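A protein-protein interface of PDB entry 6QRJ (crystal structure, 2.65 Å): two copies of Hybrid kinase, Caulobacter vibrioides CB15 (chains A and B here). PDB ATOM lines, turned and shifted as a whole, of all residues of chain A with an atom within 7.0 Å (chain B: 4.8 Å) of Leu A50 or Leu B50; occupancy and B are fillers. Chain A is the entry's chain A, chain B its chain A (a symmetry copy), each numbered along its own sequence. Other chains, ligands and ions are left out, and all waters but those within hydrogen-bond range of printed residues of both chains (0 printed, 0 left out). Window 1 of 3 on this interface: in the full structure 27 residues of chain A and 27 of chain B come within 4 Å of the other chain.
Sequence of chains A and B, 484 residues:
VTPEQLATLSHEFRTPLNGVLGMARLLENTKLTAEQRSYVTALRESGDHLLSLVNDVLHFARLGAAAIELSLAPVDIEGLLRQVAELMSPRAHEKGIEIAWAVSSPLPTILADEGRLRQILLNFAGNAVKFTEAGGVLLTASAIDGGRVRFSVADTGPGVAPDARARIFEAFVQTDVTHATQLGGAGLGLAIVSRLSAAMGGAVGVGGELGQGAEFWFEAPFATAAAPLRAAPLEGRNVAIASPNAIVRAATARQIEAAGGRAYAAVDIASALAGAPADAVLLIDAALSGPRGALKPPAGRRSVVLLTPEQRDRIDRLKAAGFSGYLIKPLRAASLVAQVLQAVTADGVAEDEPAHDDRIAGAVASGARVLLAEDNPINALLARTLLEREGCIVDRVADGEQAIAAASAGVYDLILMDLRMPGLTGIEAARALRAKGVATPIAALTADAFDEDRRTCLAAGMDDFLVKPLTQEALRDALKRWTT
The backbone carbonyl oxygen (O) of His B49 is in hydrogen-bond range of the side-chain hydroxyl (OG) of Ser B52, 2.9 Å away. O of His A49 lies within hydrogen-bond range of OG of Ser A52 (2.9 Å).
Among the printed residues, merely in contact across the chains: Glu A12 with Leu B53 (3.3 Å), Phe A13 with Leu B50 (3.8 Å), Phe A13 with Val B54 (3.8 Å), Pro A16 with Ser B46 (3.5 Å), Pro A16 with His B49 (3.8 Å), Val A20 with Gly B47 (3.99 Å), Ser A46 with Pro B16 (3.5 Å), His A49 with Pro B16 (3.8 Å), Leu A50 with Phe B13 (3.8 Å), Leu A50 with Leu B50 (3.8 Å) and Val A54 with Phe B13 (3.8 Å).
Of the printed residues of chain B, Glu A12 touches Leu B53. Of the printed residues of chain B, Val A20 touches Gly B47. Of the printed residues of chain B, Ser A46 touches Pro B16 (3.5 Å). Leu A50 touches two residues of chain B. Ser A52 touches none of the printed residues of chain B. Asp A56 touches none of the printed residues of chain B. Printed residues of chain A within 4 Å of Phe B13: Leu A50 and Val A54. Of the printed residues of chain A, Pro B16 touches Ser A46 (3.5 Å) and His A49 (3.8 Å). Of the printed residues of chain A, Leu B50 touches Phe A13 (3.8 Å) and Leu A50 (3.8 Å). The nearest residue of chain A that does not touch Leu B50 is Pro A16 (4.2 Å). The nearest printed residue of chain A that does not touch His B49 is Glu A12 (4.6 Å).
Of the 12 printed residues of chain B, 8 touch a printed residue of chain A. Hydrophobic or aromatic side chains of chain B that line the printed part of chain A: Phe B13, Pro B16, His B49, Leu B50, Leu B53 and Val B54. Of the 19 printed residues of chain A, 8 touch a printed residue of chain B. Printed residues of chain A that touch a printed residue of chain B: Glu A12, Phe A13, Pro A16, Val A20, Ser A46, His A49, Leu A50 and Val A54. Hydrophobic or aromatic side chains of chain A that line the printed part of chain B: Phe A13, Pro A16, Val A20, His A49, Leu A50 and Val A54. Among the printed residues, no Asp or Glu carboxylate lies within 4 Å of a Lys or Arg side-chain nitrogen of the other chain.
Phe A13 touches Leu B50, and with the chains exchanged Leu A50 touches Phe B13. Pro A16 touches Ser B46, and with the chains exchanged Ser A46 touches Pro B16. Pro A16 touches His B49, and with the chains exchanged His A49 touches Pro B16. Leu B50 touches its own counterpart, Leu A50. Positions printed for both chains: 13, 16, 17, 46, 47, 48, 49, 50, 51, 52, 53 and 54. Of the 11 pairs that touch across the chains among the printed residues, 9 have their exchanged pair printed and touching as well.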
ATOM      1  N   GLU A  12       8.808 -13.729  12.402  1.00  0.00           N
ATOM      2  CA  GLU A  12       8.686 -14.757  11.315  1.00  0.00           C
ATOM      3  C   GLU A  12       9.515 -16.020  11.594  1.00  0.00           C
ATOM      4  O   GLU A  12       9.021 -17.109  11.257  1.00  0.00           O
ATOM      5  CB  GLU A  12       9.112 -14.221   9.939  1.00  0.00           C
ATOM      6  CG  GLU A  12       8.135 -13.238   9.297  1.00  0.00           C
ATOM      7  CD  GLU A  12       6.717 -13.697   8.962  1.00  0.00           C
ATOM      8  OE1 GLU A  12       6.457 -14.060   7.770  1.00  0.00           O
ATOM      9  OE2 GLU A  12       5.849 -13.612   9.870  1.00  0.00           O
ATOM     10  N   PHE A  13      10.731 -15.914  12.123  1.00  0.00           N
ATOM     11  CA  PHE A  13      11.412 -17.116  12.660  1.00  0.00           C
ATOM     12  C   PHE A  13      10.647 -17.573  13.895  1.00  0.00           C
ATOM     13  O   PHE A  13      10.162 -18.710  13.902  1.00  0.00           O
ATOM     14  CB  PHE A  13      12.884 -16.851  12.899  1.00  0.00           C
ATOM     15  CG  PHE A  13      13.629 -16.975  11.605  1.00  0.00           C
ATOM     16  CD1 PHE A  13      13.556 -15.967  10.655  1.00  0.00           C
ATOM     17  CD2 PHE A  13      14.309 -18.141  11.289  1.00  0.00           C
ATOM     18  CE1 PHE A  13      14.195 -16.103   9.435  1.00  0.00           C
ATOM     19  CE2 PHE A  13      14.953 -18.273  10.071  1.00  0.00           C
ATOM     20  CZ  PHE A  13      14.886 -17.259   9.145  1.00  0.00           C
ATOM     21  N   ARG A  14      10.444 -16.695  14.867  1.00  0.00           N
ATOM     22  CA  ARG A  14       9.879 -17.139  16.156  1.00  0.00           C
ATOM     23  C   ARG A  14       8.509 -17.787  15.991  1.00  0.00           C
ATOM     24  O   ARG A  14       8.345 -18.894  16.528  1.00  0.00           O
ATOM     25  CB  ARG A  14       9.821 -16.006  17.158  1.00  0.00           C
ATOM     26  CG  ARG A  14      11.073 -16.030  18.009  1.00  0.00           C
ATOM     27  CD  ARG A  14      10.853 -15.399  19.352  1.00  0.00           C
ATOM     28  NE  ARG A  14      11.550 -14.131  19.385  1.00  0.00           N
ATOM     29  CZ  ARG A  14      12.828 -13.993  19.718  1.00  0.00           C
ATOM     30  NH1 ARG A  14      13.561 -15.051  20.034  1.00  0.00           N
ATOM     31  NH2 ARG A  14      13.377 -12.791  19.718  1.00  0.00           N
ATOM     32  N   THR A  15       7.567 -17.137  15.300  1.00  0.00           N
ATOM     33  CA  THR A  15       6.144 -17.553  15.268  1.00  0.00           C
ATOM     34  C   THR A  15       6.078 -19.031  14.903  1.00  0.00           C
ATOM     35  O   THR A  15       5.672 -19.845  15.737  1.00  0.00           O
ATOM     36  CB  THR A  15       5.308 -16.631  14.376  1.00  0.00           C
ATOM     37  OG1 THR A  15       5.323 -15.359  15.018  1.00  0.00           O
ATOM     38  CG2 THR A  15       3.877 -17.080  14.169  1.00  0.00           C
ATOM     39  N   PRO A  16       6.494 -19.462  13.695  1.00  0.00           N
ATOM     40  CA  PRO A  16       6.500 -20.886  13.390  1.00  0.00           C
ATOM     41  C   PRO A  16       7.308 -21.674  14.426  1.00  0.00           C
ATOM     42  O   PRO A  16       6.935 -22.774  14.727  1.00  0.00           O
ATOM     43  CB  PRO A  16       7.071 -20.996  11.975  1.00  0.00           C
ATOM     44  CG  PRO A  16       7.717 -19.667  11.761  1.00  0.00           C
ATOM     45  CD  PRO A  16       6.930 -18.656  12.563  1.00  0.00           C
ATOM     46  N   LEU A  17       8.366 -21.112  14.997  1.00  0.00           N
ATOM     47  CA  LEU A  17       9.163 -21.887  15.982  1.00  0.00           C
ATOM     48  C   LEU A  17       8.326 -22.103  17.235  1.00  0.00           C
ATOM     49  O   LEU A  17       8.238 -23.239  17.666  1.00  0.00           O
ATOM     50  CB  LEU A  17      10.468 -21.166  16.291  1.00  0.00           C
ATOM     51  CG  LEU A  17      11.499 -21.992  17.042  1.00  0.00           C
ATOM     52  CD1 LEU A  17      11.481 -23.444  16.607  1.00  0.00           C
ATOM     53  CD2 LEU A  17      12.872 -21.413  16.823  1.00  0.00           C
ATOM     54  N   VAL A  20       5.805 -24.955  16.554  1.00  0.00           N
ATOM     55  CA  VAL A  20       6.418 -26.290  16.796  1.00  0.00           C
ATOM     56  C   VAL A  20       6.368 -26.641  18.289  1.00  0.00           C
ATOM     57  O   VAL A  20       5.795 -27.700  18.626  1.00  0.00           O
ATOM     58  CB  VAL A  20       7.859 -26.300  16.286  1.00  0.00           C
ATOM     59  CG1 VAL A  20       8.669 -27.380  16.959  1.00  0.00           C
ATOM     60  CG2 VAL A  20       7.888 -26.447  14.773  1.00  0.00           C
ATOM     61  N   GLU A  45      13.472 -31.476  21.976  1.00  0.00           N
ATOM     62  CA  GLU A  45      14.924 -31.220  22.164  1.00  0.00           C
ATOM     63  C   GLU A  45      15.462 -30.493  20.948  1.00  0.00           C
ATOM     64  O   GLU A  45      16.148 -29.478  21.128  1.00  0.00           O
ATOM     65  CB  GLU A  45      15.801 -32.470  22.304  1.00  0.00           C
ATOM     66  CG  GLU A  45      15.638 -33.289  23.600  1.00  0.00           C
ATOM     67  CD  GLU A  45      14.944 -32.667  24.805  1.00  0.00           C
ATOM     68  OE1 GLU A  45      13.942 -33.273  25.265  1.00  0.00           O
ATOM     69  OE2 GLU A  45      15.416 -31.607  25.311  1.00  0.00           O
ATOM     70  N   SER A  46      15.234 -31.049  19.762  1.00  0.00           N
ATOM     71  CA  SER A  46      15.644 -30.392  18.491  1.00  0.00           C
ATOM     72  C   SER A  46      15.021 -28.980  18.418  1.00  0.00           C
ATOM     73  O   SER A  46      15.726 -28.025  18.082  1.00  0.00           O
ATOM     74  CB  SER A  46      15.336 -31.274  17.316  1.00  0.00           C
ATOM     75  OG  SER A  46      16.543 -31.822  16.793  1.00  0.00           O
ATOM     76  N   GLY A  47      13.762 -28.828  18.809  1.00  0.00           N
ATOM     77  CA  GLY A  47      13.129 -27.505  18.827  1.00  0.00           C
ATOM     78  C   GLY A  47      13.795 -26.558  19.809  1.00  0.00           C
ATOM     79  O   GLY A  47      14.080 -25.424  19.440  1.00  0.00           O
ATOM     80  N   ASP A  48      13.968 -26.985  21.057  1.00  0.00           N
ATOM     81  CA  ASP A  48      14.559 -26.149  22.136  1.00  0.00           C
ATOM     82  C   ASP A  48      15.948 -25.656  21.684  1.00  0.00           C
ATOM     83  O   ASP A  48      16.222 -24.442  21.834  1.00  0.00           O
ATOM     84  CB  ASP A  48      14.515 -26.899  23.469  1.00  0.00           C
ATOM     85  CG  ASP A  48      13.237 -26.707  24.304  1.00  0.00           C
ATOM     86  OD1 ASP A  48      12.535 -25.659  24.143  1.00  0.00           O
ATOM     87  OD2 ASP A  48      12.959 -27.591  25.169  1.00  0.00           O
ATOM     88  N   HIS A  49      16.731 -26.520  21.039  1.00  0.00           N
ATOM     89  CA  HIS A  49      18.108 -26.210  20.568  1.00  0.00           C
ATOM     90  C   HIS A  49      18.051 -25.083  19.534  1.00  0.00           C
ATOM     91  O   HIS A  49      18.720 -24.046  19.713  1.00  0.00           O
ATOM     92  CB  HIS A  49      18.839 -27.460  20.036  1.00  0.00           C
ATOM     93  CG  HIS A  49      20.178 -27.143  19.451  1.00  0.00           C
ATOM     94  ND1 HIS A  49      21.144 -26.430  20.143  1.00  0.00           N
ATOM     95  CD2 HIS A  49      20.703 -27.384  18.233  1.00  0.00           C
ATOM     96  CE1 HIS A  49      22.204 -26.245  19.381  1.00  0.00           C
ATOM     97  NE2 HIS A  49      21.939 -26.801  18.187  1.00  0.00           N
ATOM     98  N   LEU A  50      17.255 -25.283  18.502  1.00  0.00           N
ATOM     99  CA  LEU A  50      17.045 -24.310  17.413  1.00  0.00           C
ATOM    100  C   LEU A  50      16.603 -22.956  17.967  1.00  0.00           C
ATOM    101  O   LEU A  50      17.083 -21.953  17.478  1.00  0.00           O
ATOM    102  CB  LEU A  50      15.969 -24.908  16.514  1.00  0.00           C
ATOM    103  CG  LEU A  50      15.602 -24.102  15.287  1.00  0.00           C
ATOM    104  CD1 LEU A  50      16.773 -23.958  14.353  1.00  0.00           C
ATOM    105  CD2 LEU A  50      14.441 -24.779  14.587  1.00  0.00           C
ATOM    106  N   LEU A  51      15.693 -22.928  18.934  1.00  0.00           N
ATOM    107  CA  LEU A  51      15.222 -21.673  19.579  1.00  0.00           C
ATOM    108  C   LEU A  51      16.414 -20.956  20.208  1.00  0.00           C
ATOM    109  O   LEU A  51      16.505 -19.721  20.125  1.00  0.00           O
ATOM    110  CB  LEU A  51      14.182 -21.998  20.658  1.00  0.00           C
ATOM    111  CG  LEU A  51      13.519 -20.789  21.338  1.00  0.00           C
ATOM    112  CD1 LEU A  51      12.684 -19.980  20.359  1.00  0.00           C
ATOM    113  CD2 LEU A  51      12.652 -21.215  22.507  1.00  0.00           C
ATOM    114  N   SER A  52      17.319 -21.684  20.834  1.00  0.00           N
ATOM    115  CA  SER A  52      18.469 -21.000  21.445  1.00  0.00           C
ATOM    116  C   SER A  52      19.411 -20.501  20.329  1.00  0.00           C
ATOM    117  O   SER A  52      19.944 -19.394  20.477  1.00  0.00           O
ATOM    118  CB  SER A  52      19.113 -21.841  22.452  1.00  0.00           C
ATOM    119  OG  SER A  52      20.096 -22.611  21.816  1.00  0.00           O
ATOM    120  N   LEU A  53      19.582 -21.193  19.202  1.00  0.00           N
ATOM    121  CA  LEU A  53      20.362 -20.590  18.078  1.00  0.00           C
ATOM    122  C   LEU A  53      19.668 -19.317  17.578  1.00  0.00           C
ATOM    123  O   LEU A  53      20.348 -18.337  17.229  1.00  0.00           O
ATOM    124  CB  LEU A  53      20.540 -21.585  16.931  1.00  0.00           C
ATOM    125  CG  LEU A  53      21.397 -22.802  17.278  1.00  0.00           C
ATOM    126  CD1 LEU A  53      21.067 -23.978  16.355  1.00  0.00           C
ATOM    127  CD2 LEU A  53      22.896 -22.493  17.255  1.00  0.00           C
ATOM    128  N   VAL A  54      18.348 -19.324  17.490  1.00  0.00           N
ATOM    129  CA  VAL A  54      17.587 -18.176  16.935  1.00  0.00           C
ATOM    130  C   VAL A  54      17.689 -16.988  17.894  1.00  0.00           C
ATOM    131  O   VAL A  54      17.892 -15.865  17.410  1.00  0.00           O
ATOM    132  CB  VAL A  54      16.125 -18.575  16.724  1.00  0.00           C
ATOM    133  CG1 VAL A  54      15.191 -17.371  16.684  1.00  0.00           C
ATOM    134  CG2 VAL A  54      16.003 -19.422  15.482  1.00  0.00           C
ATOM    135  N   ASN A  55      17.470 -17.203  19.192  1.00  0.00           N
ATOM    136  CA  ASN A  55      17.555 -16.099  20.164  1.00  0.00           C
ATOM    137  C   ASN A  55      18.971 -15.547  20.102  1.00  0.00           C
ATOM    138  O   ASN A  55      19.116 -14.349  20.186  1.00  0.00           O
ATOM    139  CB  ASN A  55      17.198 -16.541  21.572  1.00  0.00           C
ATOM    140  CG  ASN A  55      15.770 -16.999  21.627  1.00  0.00           C
ATOM    141  OD1 ASN A  55      15.044 -16.812  20.662  1.00  0.00           O
ATOM    142  ND2 ASN A  55      15.375 -17.606  22.722  1.00  0.00           N
ATOM    143  N   ASP A  56      19.960 -16.406  19.932  1.00  0.00           N
ATOM    144  CA  ASP A  56      21.385 -16.009  19.985  1.00  0.00           C
ATOM    145  C   ASP A  56      21.585 -15.061  18.819  1.00  0.00           C
ATOM    146  O   ASP A  56      22.055 -13.939  19.009  1.00  0.00           O
ATOM    147  CB  ASP A  56      22.349 -17.204  19.901  1.00  0.00           C
ATOM    148  CG  ASP A  56      22.688 -17.885  21.235  1.00  0.00           C
ATOM    149  OD1 ASP A  56      22.189 -17.401  22.295  1.00  0.00           O
ATOM    150  OD2 ASP A  56      23.470 -18.907  21.212  1.00  0.00           O
ATOM    151  N   PHE B  13      21.464 -24.459  11.757  1.00  0.00           N
ATOM    152  CA  PHE B  13      20.004 -24.254  11.612  1.00  0.00           C
ATOM    153  C   PHE B  13      19.403 -25.541  11.064  1.00  0.00           C
ATOM    154  O   PHE B  13      18.542 -26.123  11.735  1.00  0.00           O
ATOM    155  CB  PHE B  13      19.703 -23.022  10.784  1.00  0.00           C
ATOM    156  CG  PHE B  13      19.816 -21.802  11.646  1.00  0.00           C
ATOM    157  CD1 PHE B  13      21.062 -21.311  12.005  1.00  0.00           C
ATOM    158  CD2 PHE B  13      18.685 -21.211  12.189  1.00  0.00           C
ATOM    159  CE1 PHE B  13      21.172 -20.219  12.848  1.00  0.00           C
ATOM    160  CE2 PHE B  13      18.795 -20.116  13.027  1.00  0.00           C
ATOM    161  CZ  PHE B  13      20.037 -19.629  13.362  1.00  0.00           C
ATOM    162  N   PRO B  16      19.075 -29.378  13.520  1.00  0.00           N
ATOM    163  CA  PRO B  16      17.918 -29.424  14.405  1.00  0.00           C
ATOM    164  C   PRO B  16      16.611 -29.273  13.619  1.00  0.00           C
ATOM    165  O   PRO B  16      15.646 -29.883  13.992  1.00  0.00           O
ATOM    166  CB  PRO B  16      18.139 -28.302  15.421  1.00  0.00           C
ATOM    167  CG  PRO B  16      19.192 -27.460  14.780  1.00  0.00           C
ATOM    168  CD  PRO B  16      20.049 -28.381  13.942  1.00  0.00           C
ATOM    169  N   LEU B  17      16.585 -28.517  12.529  1.00  0.00           N
ATOM    170  CA  LEU B  17      15.310 -28.352  11.785  1.00  0.00           C
ATOM    171  C   LEU B  17      14.939 -29.680  11.140  1.00  0.00           C
ATOM    172  O   LEU B  17      13.810 -30.100  11.322  1.00  0.00           O
ATOM    173  CB  LEU B  17      15.441 -27.240  10.753  1.00  0.00           C
ATOM    174  CG  LEU B  17      14.130 -26.770  10.143  1.00  0.00           C
ATOM    175  CD1 LEU B  17      13.002 -26.782  11.154  1.00  0.00           C
ATOM    176  CD2 LEU B  17      14.298 -25.380   9.586  1.00  0.00           C
ATOM    177  N   SER B  46       4.016 -25.864  10.633  1.00  0.00           N
ATOM    178  CA  SER B  46       4.915 -24.848  11.246  1.00  0.00           C
ATOM    179  C   SER B  46       6.381 -25.182  10.894  1.00  0.00           C
ATOM    180  O   SER B  46       7.128 -24.283  10.500  1.00  0.00           O
ATOM    181  CB  SER B  46       4.638 -24.713  12.715  1.00  0.00           C
ATOM    182  OG  SER B  46       3.965 -23.483  12.969  1.00  0.00           O
ATOM    183  N   GLY B  47       6.767 -26.451  10.943  1.00  0.00           N
ATOM    184  CA  GLY B  47       8.126 -26.846  10.559  1.00  0.00           C
ATOM    185  C   GLY B  47       8.418 -26.570   9.095  1.00  0.00           C
ATOM    186  O   GLY B  47       9.463 -26.004   8.795  1.00  0.00           O
ATOM    187  N   ASP B  48       7.551 -27.029   8.197  1.00  0.00           N
ATOM    188  CA  ASP B  48       7.734 -26.877   6.728  1.00  0.00           C
ATOM    189  C   ASP B  48       7.901 -25.381   6.396  1.00  0.00           C
ATOM    190  O   ASP B  48       8.840 -25.046   5.636  1.00  0.00           O
ATOM    191  CB  ASP B  48       6.618 -27.608   5.979  1.00  0.00           C
ATOM    192  CG  ASP B  48       6.888 -29.087   5.651  1.00  0.00           C
ATOM    193  OD1 ASP B  48       8.088 -29.499   5.561  1.00  0.00           O
ATOM    194  OD2 ASP B  48       5.889 -29.834   5.428  1.00  0.00           O
ATOM    195  N   HIS B  49       7.121 -24.513   7.040  1.00  0.00           N
ATOM    196  CA  HIS B  49       7.137 -23.043   6.809  1.00  0.00           C
ATOM    197  C   HIS B  49       8.513 -22.485   7.180  1.00  0.00           C
ATOM    198  O   HIS B  49       9.163 -21.836   6.337  1.00  0.00           O
ATOM    199  CB  HIS B  49       5.992 -22.323   7.551  1.00  0.00           C
ATOM    200  CG  HIS B  49       6.066 -20.835   7.425  1.00  0.00           C
ATOM    201  ND1 HIS B  49       6.159 -20.194   6.199  1.00  0.00           N
ATOM    202  CD2 HIS B  49       6.116 -19.859   8.353  1.00  0.00           C
ATOM    203  CE1 HIS B  49       6.264 -18.891   6.375  1.00  0.00           C
ATOM    204  NE2 HIS B  49       6.269 -18.667   7.700  1.00  0.00           N
ATOM    205  N   LEU B  50       8.940 -22.756   8.398  1.00  0.00           N
ATOM    206  CA  LEU B  50      10.246 -22.329   8.935  1.00  0.00           C
ATOM    207  C   LEU B  50      11.388 -22.789   8.029  1.00  0.00           C
ATOM    208  O   LEU B  50      12.300 -22.015   7.818  1.00  0.00           O
ATOM    209  CB  LEU B  50      10.361 -22.960  10.318  1.00  0.00           C
ATOM    210  CG  LEU B  50      11.616 -22.632  11.098  1.00  0.00           C
ATOM    211  CD1 LEU B  50      11.709 -21.160  11.396  1.00  0.00           C
ATOM    212  CD2 LEU B  50      11.617 -23.436  12.382  1.00  0.00           C
ATOM    213  N   LEU B  51      11.355 -24.022   7.537  1.00  0.00           N
ATOM    214  CA  LEU B  51      12.385 -24.563   6.610  1.00  0.00           C
ATOM    215  C   LEU B  51      12.435 -23.693   5.356  1.00  0.00           C
ATOM    216  O   LEU B  51      13.530 -23.413   4.842  1.00  0.00           O
ATOM    217  CB  LEU B  51      12.041 -26.007   6.228  1.00  0.00           C
ATOM    218  CG  LEU B  51      13.078 -26.738   5.360  1.00  0.00           C
ATOM    219  CD1 LEU B  51      14.392 -26.934   6.098  1.00  0.00           C
ATOM    220  CD2 LEU B  51      12.558 -28.083   4.888  1.00  0.00           C
ATOM    221  N   SER B  52      11.294 -23.267   4.849  1.00  0.00           N
ATOM    222  CA  SER B  52      11.334 -22.430   3.639  1.00  0.00           C
ATOM    223  C   SER B  52      11.876 -21.034   4.008  1.00  0.00           C
ATOM    224  O   SER B  52      12.642 -20.482   3.206  1.00  0.00           O
ATOM    225  CB  SER B  52      10.040 -22.419   2.959  1.00  0.00           C
ATOM    226  OG  SER B  52       9.279 -21.367   3.484  1.00  0.00           O
ATOM    227  N   LEU B  53      11.604 -20.471   5.186  1.00  0.00           N
ATOM    228  CA  LEU B  53      12.291 -19.200   5.572  1.00  0.00           C
ATOM    229  C   LEU B  53      13.805 -19.424   5.659  1.00  0.00           C
ATOM    230  O   LEU B  53      14.586 -18.538   5.272  1.00  0.00           O
ATOM    231  CB  LEU B  53      11.755 -18.661   6.898  1.00  0.00           C
ATOM    232  CG  LEU B  53      10.294 -18.217   6.856  1.00  0.00           C
ATOM    233  CD1 LEU B  53       9.675 -18.252   8.256  1.00  0.00           C
ATOM    234  CD2 LEU B  53      10.115 -16.838   6.214  1.00  0.00           C
ATOM    235  N   VAL B  54      14.235 -20.555   6.194  1.00  0.00           N
ATOM    236  CA  VAL B  54      15.679 -20.831   6.406  1.00  0.00           C
ATOM    237  C   VAL B  54      16.365 -21.012   5.050  1.00  0.00           C
ATOM    238  O   VAL B  54      17.466 -20.469   4.878  1.00  0.00           O
ATOM    239  CB  VAL B  54      15.847 -22.083   7.267  1.00  0.00           C
ATOM    240  CG1 VAL B  54      17.214 -22.735   7.090  1.00  0.00           C
ATOM    241  CG2 VAL B  54      15.568 -21.749   8.712  1.00  0.00           C
